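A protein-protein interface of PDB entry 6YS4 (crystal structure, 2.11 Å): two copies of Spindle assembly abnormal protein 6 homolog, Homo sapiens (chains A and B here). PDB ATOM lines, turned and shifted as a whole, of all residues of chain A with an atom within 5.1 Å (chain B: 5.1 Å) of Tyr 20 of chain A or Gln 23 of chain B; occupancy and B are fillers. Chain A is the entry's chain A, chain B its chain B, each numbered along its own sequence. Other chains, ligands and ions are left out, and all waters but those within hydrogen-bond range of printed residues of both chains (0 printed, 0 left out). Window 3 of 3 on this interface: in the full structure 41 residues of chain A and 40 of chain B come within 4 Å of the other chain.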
ATOM      1  N   ALA A  16      24.160  -5.712 -17.888  1.00  0.00           N
ATOM      2  CA  ALA A  16      22.794  -5.236 -17.700  1.00  0.00           C
ATOM      3  C   ALA A  16      22.404  -5.302 -16.193  1.00  0.00           C
ATOM      4  O   ALA A  16      21.722  -4.391 -15.727  1.00  0.00           O
ATOM      5  CB  ALA A  16      21.826  -6.045 -18.542  1.00  0.00           C
ATOM      6  N   GLN A  17      22.864  -6.347 -15.445  1.00  0.00           N
ATOM      7  CA  GLN A  17      22.615  -6.474 -14.010  1.00  0.00           C
ATOM      8  C   GLN A  17      23.342  -5.357 -13.248  1.00  0.00           C
ATOM      9  O   GLN A  17      22.798  -4.818 -12.293  1.00  0.00           O
ATOM     10  CB  GLN A  17      23.038  -7.878 -13.506  1.00  0.00           C
ATOM     11  CG  GLN A  17      23.061  -8.057 -11.969  1.00  0.00           C
ATOM     12  CD  GLN A  17      21.714  -8.245 -11.310  1.00  0.00           C
ATOM     13  OE1 GLN A  17      20.648  -8.160 -11.932  1.00  0.00           O
ATOM     14  NE2 GLN A  17      21.744  -8.511 -10.014  1.00  0.00           N
ATOM     15  N   VAL A  18      24.571  -5.021 -13.672  1.00  0.00           N
ATOM     16  CA  VAL A  18      25.384  -3.962 -13.051  1.00  0.00           C
ATOM     17  C   VAL A  18      24.662  -2.603 -13.232  1.00  0.00           C
ATOM     18  O   VAL A  18      24.555  -1.833 -12.289  1.00  0.00           O
ATOM     19  CB  VAL A  18      26.845  -3.956 -13.639  1.00  0.00           C
ATOM     20  CG1 VAL A  18      27.654  -2.765 -13.121  1.00  0.00           C
ATOM     21  CG2 VAL A  18      27.574  -5.253 -13.312  1.00  0.00           C
ATOM     22  N   GLN A  19      24.157  -2.345 -14.445  1.00  0.00           N
ATOM     23  CA  GLN A  19      23.448  -1.132 -14.803  1.00  0.00           C
ATOM     24  C   GLN A  19      22.148  -0.966 -14.033  1.00  0.00           C
ATOM     25  O   GLN A  19      21.855   0.154 -13.584  1.00  0.00           O
ATOM     26  CB  GLN A  19      23.240  -1.036 -16.336  1.00  0.00           C
ATOM     27  CG  GLN A  19      24.445  -0.466 -17.122  1.00  0.00           C
ATOM     28  CD  GLN A  19      25.187   0.705 -16.475  1.00  0.00           C
ATOM     29  OE1 GLN A  19      24.606   1.723 -16.086  1.00  0.00           O
ATOM     30  NE2 GLN A  19      26.491   0.577 -16.333  1.00  0.00           N
ATOM     31  N   TYR A  20      21.409  -2.087 -13.829  1.00  0.00           N
ATOM     32  CA  TYR A  20      20.179  -2.101 -13.048  1.00  0.00           C
ATOM     33  C   TYR A  20      20.456  -1.661 -11.629  1.00  0.00           C
ATOM     34  O   TYR A  20      19.674  -0.855 -11.100  1.00  0.00           O
ATOM     35  CB  TYR A  20      19.461  -3.480 -13.021  1.00  0.00           C
ATOM     36  CG  TYR A  20      18.555  -3.631 -11.788  1.00  0.00           C
ATOM     37  CD1 TYR A  20      17.367  -2.895 -11.666  1.00  0.00           C
ATOM     38  CD2 TYR A  20      18.913  -4.467 -10.726  1.00  0.00           C
ATOM     39  CE1 TYR A  20      16.580  -2.968 -10.506  1.00  0.00           C
ATOM     40  CE2 TYR A  20      18.113  -4.574  -9.583  1.00  0.00           C
ATOM     41  CZ  TYR A  20      16.955  -3.814  -9.475  1.00  0.00           C
ATOM     42  OH  TYR A  20      16.168  -3.907  -8.351  1.00  0.00           O
ATOM     43  N   GLN A  21      21.476  -2.306 -10.961  1.00  0.00           N
ATOM     44  CA  GLN A  21      21.835  -2.004  -9.565  1.00  0.00           C
ATOM     45  C   GLN A  21      22.184  -0.516  -9.469  1.00  0.00           C
ATOM     46  O   GLN A  21      21.699   0.142  -8.574  1.00  0.00           O
ATOM     47  CB  GLN A  21      23.055  -2.824  -9.070  1.00  0.00           C
ATOM     48  CG  GLN A  21      22.863  -4.315  -8.809  1.00  0.00           C
ATOM     49  CD  GLN A  21      24.196  -4.985  -8.432  1.00  0.00           C
ATOM     50  OE1 GLN A  21      24.421  -5.408  -7.283  1.00  0.00           O
ATOM     51  NE2 GLN A  21      25.128  -5.090  -9.390  1.00  0.00           N
ATOM     52  N   GLN A  22      22.968   0.028 -10.440  1.00  0.00           N
ATOM     53  CA  GLN A  22      23.348   1.455 -10.426  1.00  0.00           C
ATOM     54  C   GLN A  22      22.128   2.387 -10.533  1.00  0.00           C
ATOM     55  O   GLN A  22      22.056   3.371  -9.795  1.00  0.00           O
ATOM     56  CB  GLN A  22      24.356   1.766 -11.535  1.00  0.00           C
ATOM     57  CG  GLN A  22      25.740   1.155 -11.344  1.00  0.00           C
ATOM     58  CD  GLN A  22      26.652   1.397 -12.544  1.00  0.00           C
ATOM     59  OE1 GLN A  22      26.359   2.198 -13.447  1.00  0.00           O
ATOM     60  NE2 GLN A  22      27.795   0.717 -12.580  1.00  0.00           N
ATOM     61  N   GLN A  23      21.173   2.065 -11.435  1.00  0.00           N
ATOM     62  CA  GLN A  23      19.934   2.816 -11.636  1.00  0.00           C
ATOM     63  C   GLN A  23      18.999   2.719 -10.420  1.00  0.00           C
ATOM     64  O   GLN A  23      18.316   3.673 -10.114  1.00  0.00           O
ATOM     65  CB  GLN A  23      19.202   2.390 -12.914  1.00  0.00           C
ATOM     66  CG  GLN A  23      19.811   2.999 -14.178  1.00  0.00           C
ATOM     67  CD  GLN A  23      19.552   2.243 -15.483  1.00  0.00           C
ATOM     68  OE1 GLN A  23      18.708   1.343 -15.584  1.00  0.00           O
ATOM     69  NE2 GLN A  23      20.294   2.601 -16.531  1.00  0.00           N
ATOM     70  N   HIS A  24      18.978   1.581  -9.738  1.00  0.00           N
ATOM     71  CA  HIS A  24      18.172   1.397  -8.525  1.00  0.00           C
ATOM     72  C   HIS A  24      18.723   2.262  -7.383  1.00  0.00           C
ATOM     73  O   HIS A  24      17.950   2.888  -6.675  1.00  0.00           O
ATOM     74  CB  HIS A  24      18.136  -0.074  -8.128  1.00  0.00           C
ATOM     75  CG  HIS A  24      16.883  -0.462  -7.423  1.00  0.00           C
ATOM     76  ND1 HIS A  24      15.659  -0.468  -8.079  1.00  0.00           N
ATOM     77  CD2 HIS A  24      16.707  -0.928  -6.153  1.00  0.00           C
ATOM     78  CE1 HIS A  24      14.775  -0.907  -7.176  1.00  0.00           C
ATOM     79  NE2 HIS A  24      15.360  -1.218  -6.012  1.00  0.00           N
ATOM     80  N   GLU A  25      20.055   2.327  -7.241  1.00  0.00           N
ATOM     81  CA  GLU A  25      20.737   3.156  -6.246  1.00  0.00           C
ATOM     82  C   GLU A  25      20.542   4.642  -6.553  1.00  0.00           C
ATOM     83  O   GLU A  25      20.321   5.413  -5.644  1.00  0.00           O
ATOM     84  CB  GLU A  25      22.233   2.805  -6.193  1.00  0.00           C
ATOM     85  CG  GLU A  25      22.529   1.599  -5.323  1.00  0.00           C
ATOM     86  CD  GLU A  25      23.733   0.748  -5.692  1.00  0.00           C
ATOM     87  OE1 GLU A  25      23.633  -0.493  -5.548  1.00  0.00           O
ATOM     88  OE2 GLU A  25      24.768   1.308  -6.123  1.00  0.00           O
ATOM     89  N   GLN B  19      11.526  -7.462 -15.058  1.00  0.00           N
ATOM     90  CA  GLN B  19      11.803  -7.587 -13.633  1.00  0.00           C
ATOM     91  C   GLN B  19      12.421  -6.345 -13.031  1.00  0.00           C
ATOM     92  O   GLN B  19      11.999  -5.938 -11.960  1.00  0.00           O
ATOM     93  CB  GLN B  19      12.689  -8.797 -13.347  1.00  0.00           C
ATOM     94  CG  GLN B  19      11.927 -10.115 -13.172  1.00  0.00           C
ATOM     95  CD  GLN B  19      11.336 -10.243 -11.788  1.00  0.00           C
ATOM     96  OE1 GLN B  19      10.325  -9.612 -11.471  1.00  0.00           O
ATOM     97  NE2 GLN B  19      11.961 -11.049 -10.931  1.00  0.00           N
ATOM     98  N   TYR B  20      13.421  -5.747 -13.718  1.00  0.00           N
ATOM     99  CA  TYR B  20      14.144  -4.563 -13.299  1.00  0.00           C
ATOM    100  C   TYR B  20      13.158  -3.401 -13.154  1.00  0.00           C
ATOM    101  O   TYR B  20      13.182  -2.676 -12.143  1.00  0.00           O
ATOM    102  CB  TYR B  20      15.319  -4.248 -14.274  1.00  0.00           C
ATOM    103  CG  TYR B  20      16.442  -5.294 -14.307  1.00  0.00           C
ATOM    104  CD1 TYR B  20      16.644  -6.173 -13.235  1.00  0.00           C
ATOM    105  CD2 TYR B  20      17.292  -5.415 -15.419  1.00  0.00           C
ATOM    106  CE1 TYR B  20      17.647  -7.147 -13.268  1.00  0.00           C
ATOM    107  CE2 TYR B  20      18.330  -6.356 -15.441  1.00  0.00           C
ATOM    108  CZ  TYR B  20      18.489  -7.237 -14.368  1.00  0.00           C
ATOM    109  OH  TYR B  20      19.472  -8.202 -14.351  1.00  0.00           O
ATOM    110  N   GLN B  21      12.253  -3.291 -14.151  1.00  0.00           N
ATOM    111  CA  GLN B  21      11.203  -2.286 -14.232  1.00  0.00           C
ATOM    112  C   GLN B  21      10.176  -2.450 -13.122  1.00  0.00           C
ATOM    113  O   GLN B  21       9.861  -1.476 -12.460  1.00  0.00           O
ATOM    114  CB  GLN B  21      10.563  -2.284 -15.642  1.00  0.00           C
ATOM    115  CG  GLN B  21      10.104  -0.893 -16.114  1.00  0.00           C
ATOM    116  CD  GLN B  21      11.169   0.177 -15.957  1.00  0.00           C
ATOM    117  OE1 GLN B  21      12.266   0.081 -16.516  1.00  0.00           O
ATOM    118  NE2 GLN B  21      10.875   1.212 -15.180  1.00  0.00           N
ATOM    119  N   GLN B  22       9.758  -3.685 -12.823  1.00  0.00           N
ATOM    120  CA  GLN B  22       8.828  -3.928 -11.716  1.00  0.00           C
ATOM    121  C   GLN B  22       9.488  -3.550 -10.373  1.00  0.00           C
ATOM    122  O   GLN B  22       8.831  -2.972  -9.528  1.00  0.00           O
ATOM    123  CB  GLN B  22       8.382  -5.385 -11.674  1.00  0.00           C
ATOM    124  CG  GLN B  22       7.453  -5.825 -12.809  1.00  0.00           C
ATOM    125  CD  GLN B  22       7.215  -7.340 -12.850  1.00  0.00           C
ATOM    126  OE1 GLN B  22       7.569  -8.096 -11.931  1.00  0.00           O
ATOM    127  NE2 GLN B  22       6.604  -7.818 -13.929  1.00  0.00           N
ATOM    128  N   GLN B  23      10.793  -3.869 -10.211  1.00  0.00           N
ATOM    129  CA  GLN B  23      11.587  -3.568  -9.028  1.00  0.00           C
ATOM    130  C   GLN B  23      11.814  -2.085  -8.849  1.00  0.00           C
ATOM    131  O   GLN B  23      11.829  -1.635  -7.728  1.00  0.00           O
ATOM    132  CB  GLN B  23      12.910  -4.350  -9.039  1.00  0.00           C
ATOM    133  CG  GLN B  23      12.736  -5.807  -8.532  1.00  0.00           C
ATOM    134  CD  GLN B  23      13.841  -6.782  -8.921  1.00  0.00           C
ATOM    135  OE1 GLN B  23      14.936  -6.400  -9.338  1.00  0.00           O
ATOM    136  NE2 GLN B  23      13.568  -8.085  -8.788  1.00  0.00           N
ATOM    137  N   HIS B  24      11.991  -1.334  -9.960  1.00  0.00           N
ATOM    138  CA  HIS B  24      12.207   0.110  -9.937  1.00  0.00           C
ATOM    139  C   HIS B  24      10.943   0.799  -9.445  1.00  0.00           C
ATOM    140  O   HIS B  24      11.012   1.690  -8.602  1.00  0.00           O
ATOM    141  CB  HIS B  24      12.583   0.594 -11.334  1.00  0.00           C
ATOM    142  CG  HIS B  24      13.351   1.874 -11.356  1.00  0.00           C
ATOM    143  ND1 HIS B  24      14.652   1.943 -10.881  1.00  0.00           N
ATOM    144  CD2 HIS B  24      13.011   3.074 -11.886  1.00  0.00           C
ATOM    145  CE1 HIS B  24      15.043   3.188 -11.096  1.00  0.00           C
ATOM    146  NE2 HIS B  24      14.094   3.902 -11.706  1.00  0.00           N
ATOM    147  N   GLU B  25       9.782   0.345  -9.945  1.00  0.00           N
ATOM    148  CA  GLU B  25       8.473   0.852  -9.566  1.00  0.00           C
ATOM    149  C   GLU B  25       8.167   0.544  -8.106  1.00  0.00           C
ATOM    150  O   GLU B  25       7.673   1.416  -7.389  1.00  0.00           O
ATOM    151  CB  GLU B  25       7.390   0.294 -10.492  1.00  0.00           C
ATOM    152  CG  GLU B  25       7.326   1.053 -11.827  1.00  0.00           C
ATOM    153  CD  GLU B  25       6.914   0.292 -13.076  1.00  0.00           C
ATOM    154  OE1 GLU B  25       7.478   0.581 -14.159  1.00  0.00           O
ATOM    155  OE2 GLU B  25       6.028  -0.588 -12.977  1.00  0.00           O
ATOM    156  N   GLN B  26       8.450  -0.695  -7.665  1.00  0.00           N
ATOM    157  CA  GLN B  26       8.217  -1.128  -6.281  1.00  0.00           C
ATOM    158  C   GLN B  26       9.069  -0.339  -5.274  1.00  0.00           C
ATOM    159  O   GLN B  26       8.523   0.096  -4.257  1.00  0.00           O
ATOM    160  CB  GLN B  26       8.409  -2.629  -6.140  1.00  0.00           C
ATOM    161  CG  GLN B  26       7.813  -3.219  -4.837  1.00  0.00           C
ATOM    162  CD  GLN B  26       6.342  -2.917  -4.632  1.00  0.00           C
ATOM    163  OE1 GLN B  26       5.941  -2.259  -3.664  1.00  0.00           O
ATOM    164  NE2 GLN B  26       5.503  -3.380  -5.551  1.00  0.00           N
ATOM    165  N   GLN B  27      10.365  -0.082  -5.587  1.00  0.00           N
ATOM    166  CA  GLN B  27      11.208   0.741  -4.716  1.00  0.00           C
ATOM    167  C   GLN B  27      10.642   2.184  -4.564  1.00  0.00           C
ATOM    168  O   GLN B  27      10.607   2.710  -3.468  1.00  0.00           O
ATOM    169  CB  GLN B  27      12.667   0.767  -5.201  1.00  0.00           C
ATOM    170  CG  GLN B  27      13.517   1.825  -4.473  1.00  0.00           C
ATOM    171  CD  GLN B  27      14.953   1.858  -4.920  1.00  0.00           C
ATOM    172  OE1 GLN B  27      15.314   2.406  -5.993  1.00  0.00           O
ATOM    173  NE2 GLN B  27      15.797   1.264  -4.091  1.00  0.00           N
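Printed residues of chain B within 4 Å of Tyr 20 of chain A: Tyr 20 (3.5 Å) and Gln 23 (3.0 Å).
Of chain A, only Tyr 20 (3.0 Å) and His 24 (3.1 Å) come within 4 Å of Gln 23 of chain B.
Of the printed residues of chain B, Gln 23 of chain A touches His 24.
Of the printed residues of chain B, Gln 17 of chain A touches Tyr 20.
Of the printed residues of chain A, Tyr 20 of chain B touches Ala 16 (3.9 Å), Gln 17 (2.7 Å) and Tyr 20 (3.5 Å).
Of the printed residues of chain B, Ala 16 of chain A touches Tyr 20 (3.9 Å).
Printed residues of chain A within 4 Å of Gln 27 of chain B: His 24 (2.8 Å).
Gln 26 of chain B touches none of the printed residues of chain A.
Gln 19 of chain B touches none of the printed residues of chain A.
The nearest printed residue of chain B that does not touch Tyr 20 of chain A is His 24 of chain B (4.9 Å).
The nearest printed residue of chain A that does not touch Gln 23 of chain B is Gln 17 of chain A (6.5 Å).
The nearest printed residue of chain B that does not touch Gln 23 of chain A is Gln 27 of chain B (5.3 Å).
Of the 10 printed residues of chain A, 5 touch a printed residue of chain B.
Hydrophobic or aromatic side chains of chain A that line the printed part of chain B: Tyr 20 and His 24.
Among the printed residues, merely in contact across the chains: Ala 16 of chain A with Tyr 20 of chain B (3.9 Å), Tyr 20 of chain A with Tyr 20 of chain B (3.5 Å), Gln 23 of chain A with His 24 of chain B (3.5 Å), His 24 of chain A with Gln 23 of chain B (3.1 Å) and His 24 of chain A with His 24 of chain B (3.8 Å).
Tyr 20 of chain B touches its own counterpart, Tyr 20 of chain A.
Tyr 20 of chain A touches Gln 23 of chain B, but with the chains exchanged Gln 23 of chain A does not touch Tyr 20 of chain B (6.7 Å).
Gln 23 of chain A touches His 24 of chain B, and with the chains exchanged His 24 of chain A touches Gln 23 of chain B.
His 24 of chain B touches its own counterpart, His 24 of chain A.
Of the 8 pairs that touch across the chains among the printed residues, 4 have their exchanged pair printed and touching as well.
The side-chain hydroxyl of Tyr 20 of chain A is in hydrogen-bond range of a ring nitrogen (ND1) of His 24 of chain A (3.5 Å).
The backbone carbonyl oxygen (O) of His 24 of chain A lies close to the side-chain amide oxygen (OE1) of Gln 27 of chain B.
The side-chain amide oxygen of Gln 17 of chain A lies within hydrogen-bond range of the side-chain hydroxyl of Tyr 20 of chain B, at 2.7 Å.
OH of Tyr 20 of chain A is in hydrogen-bond range of OE1 of Gln 23 of chain B, at 3.0 Å.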
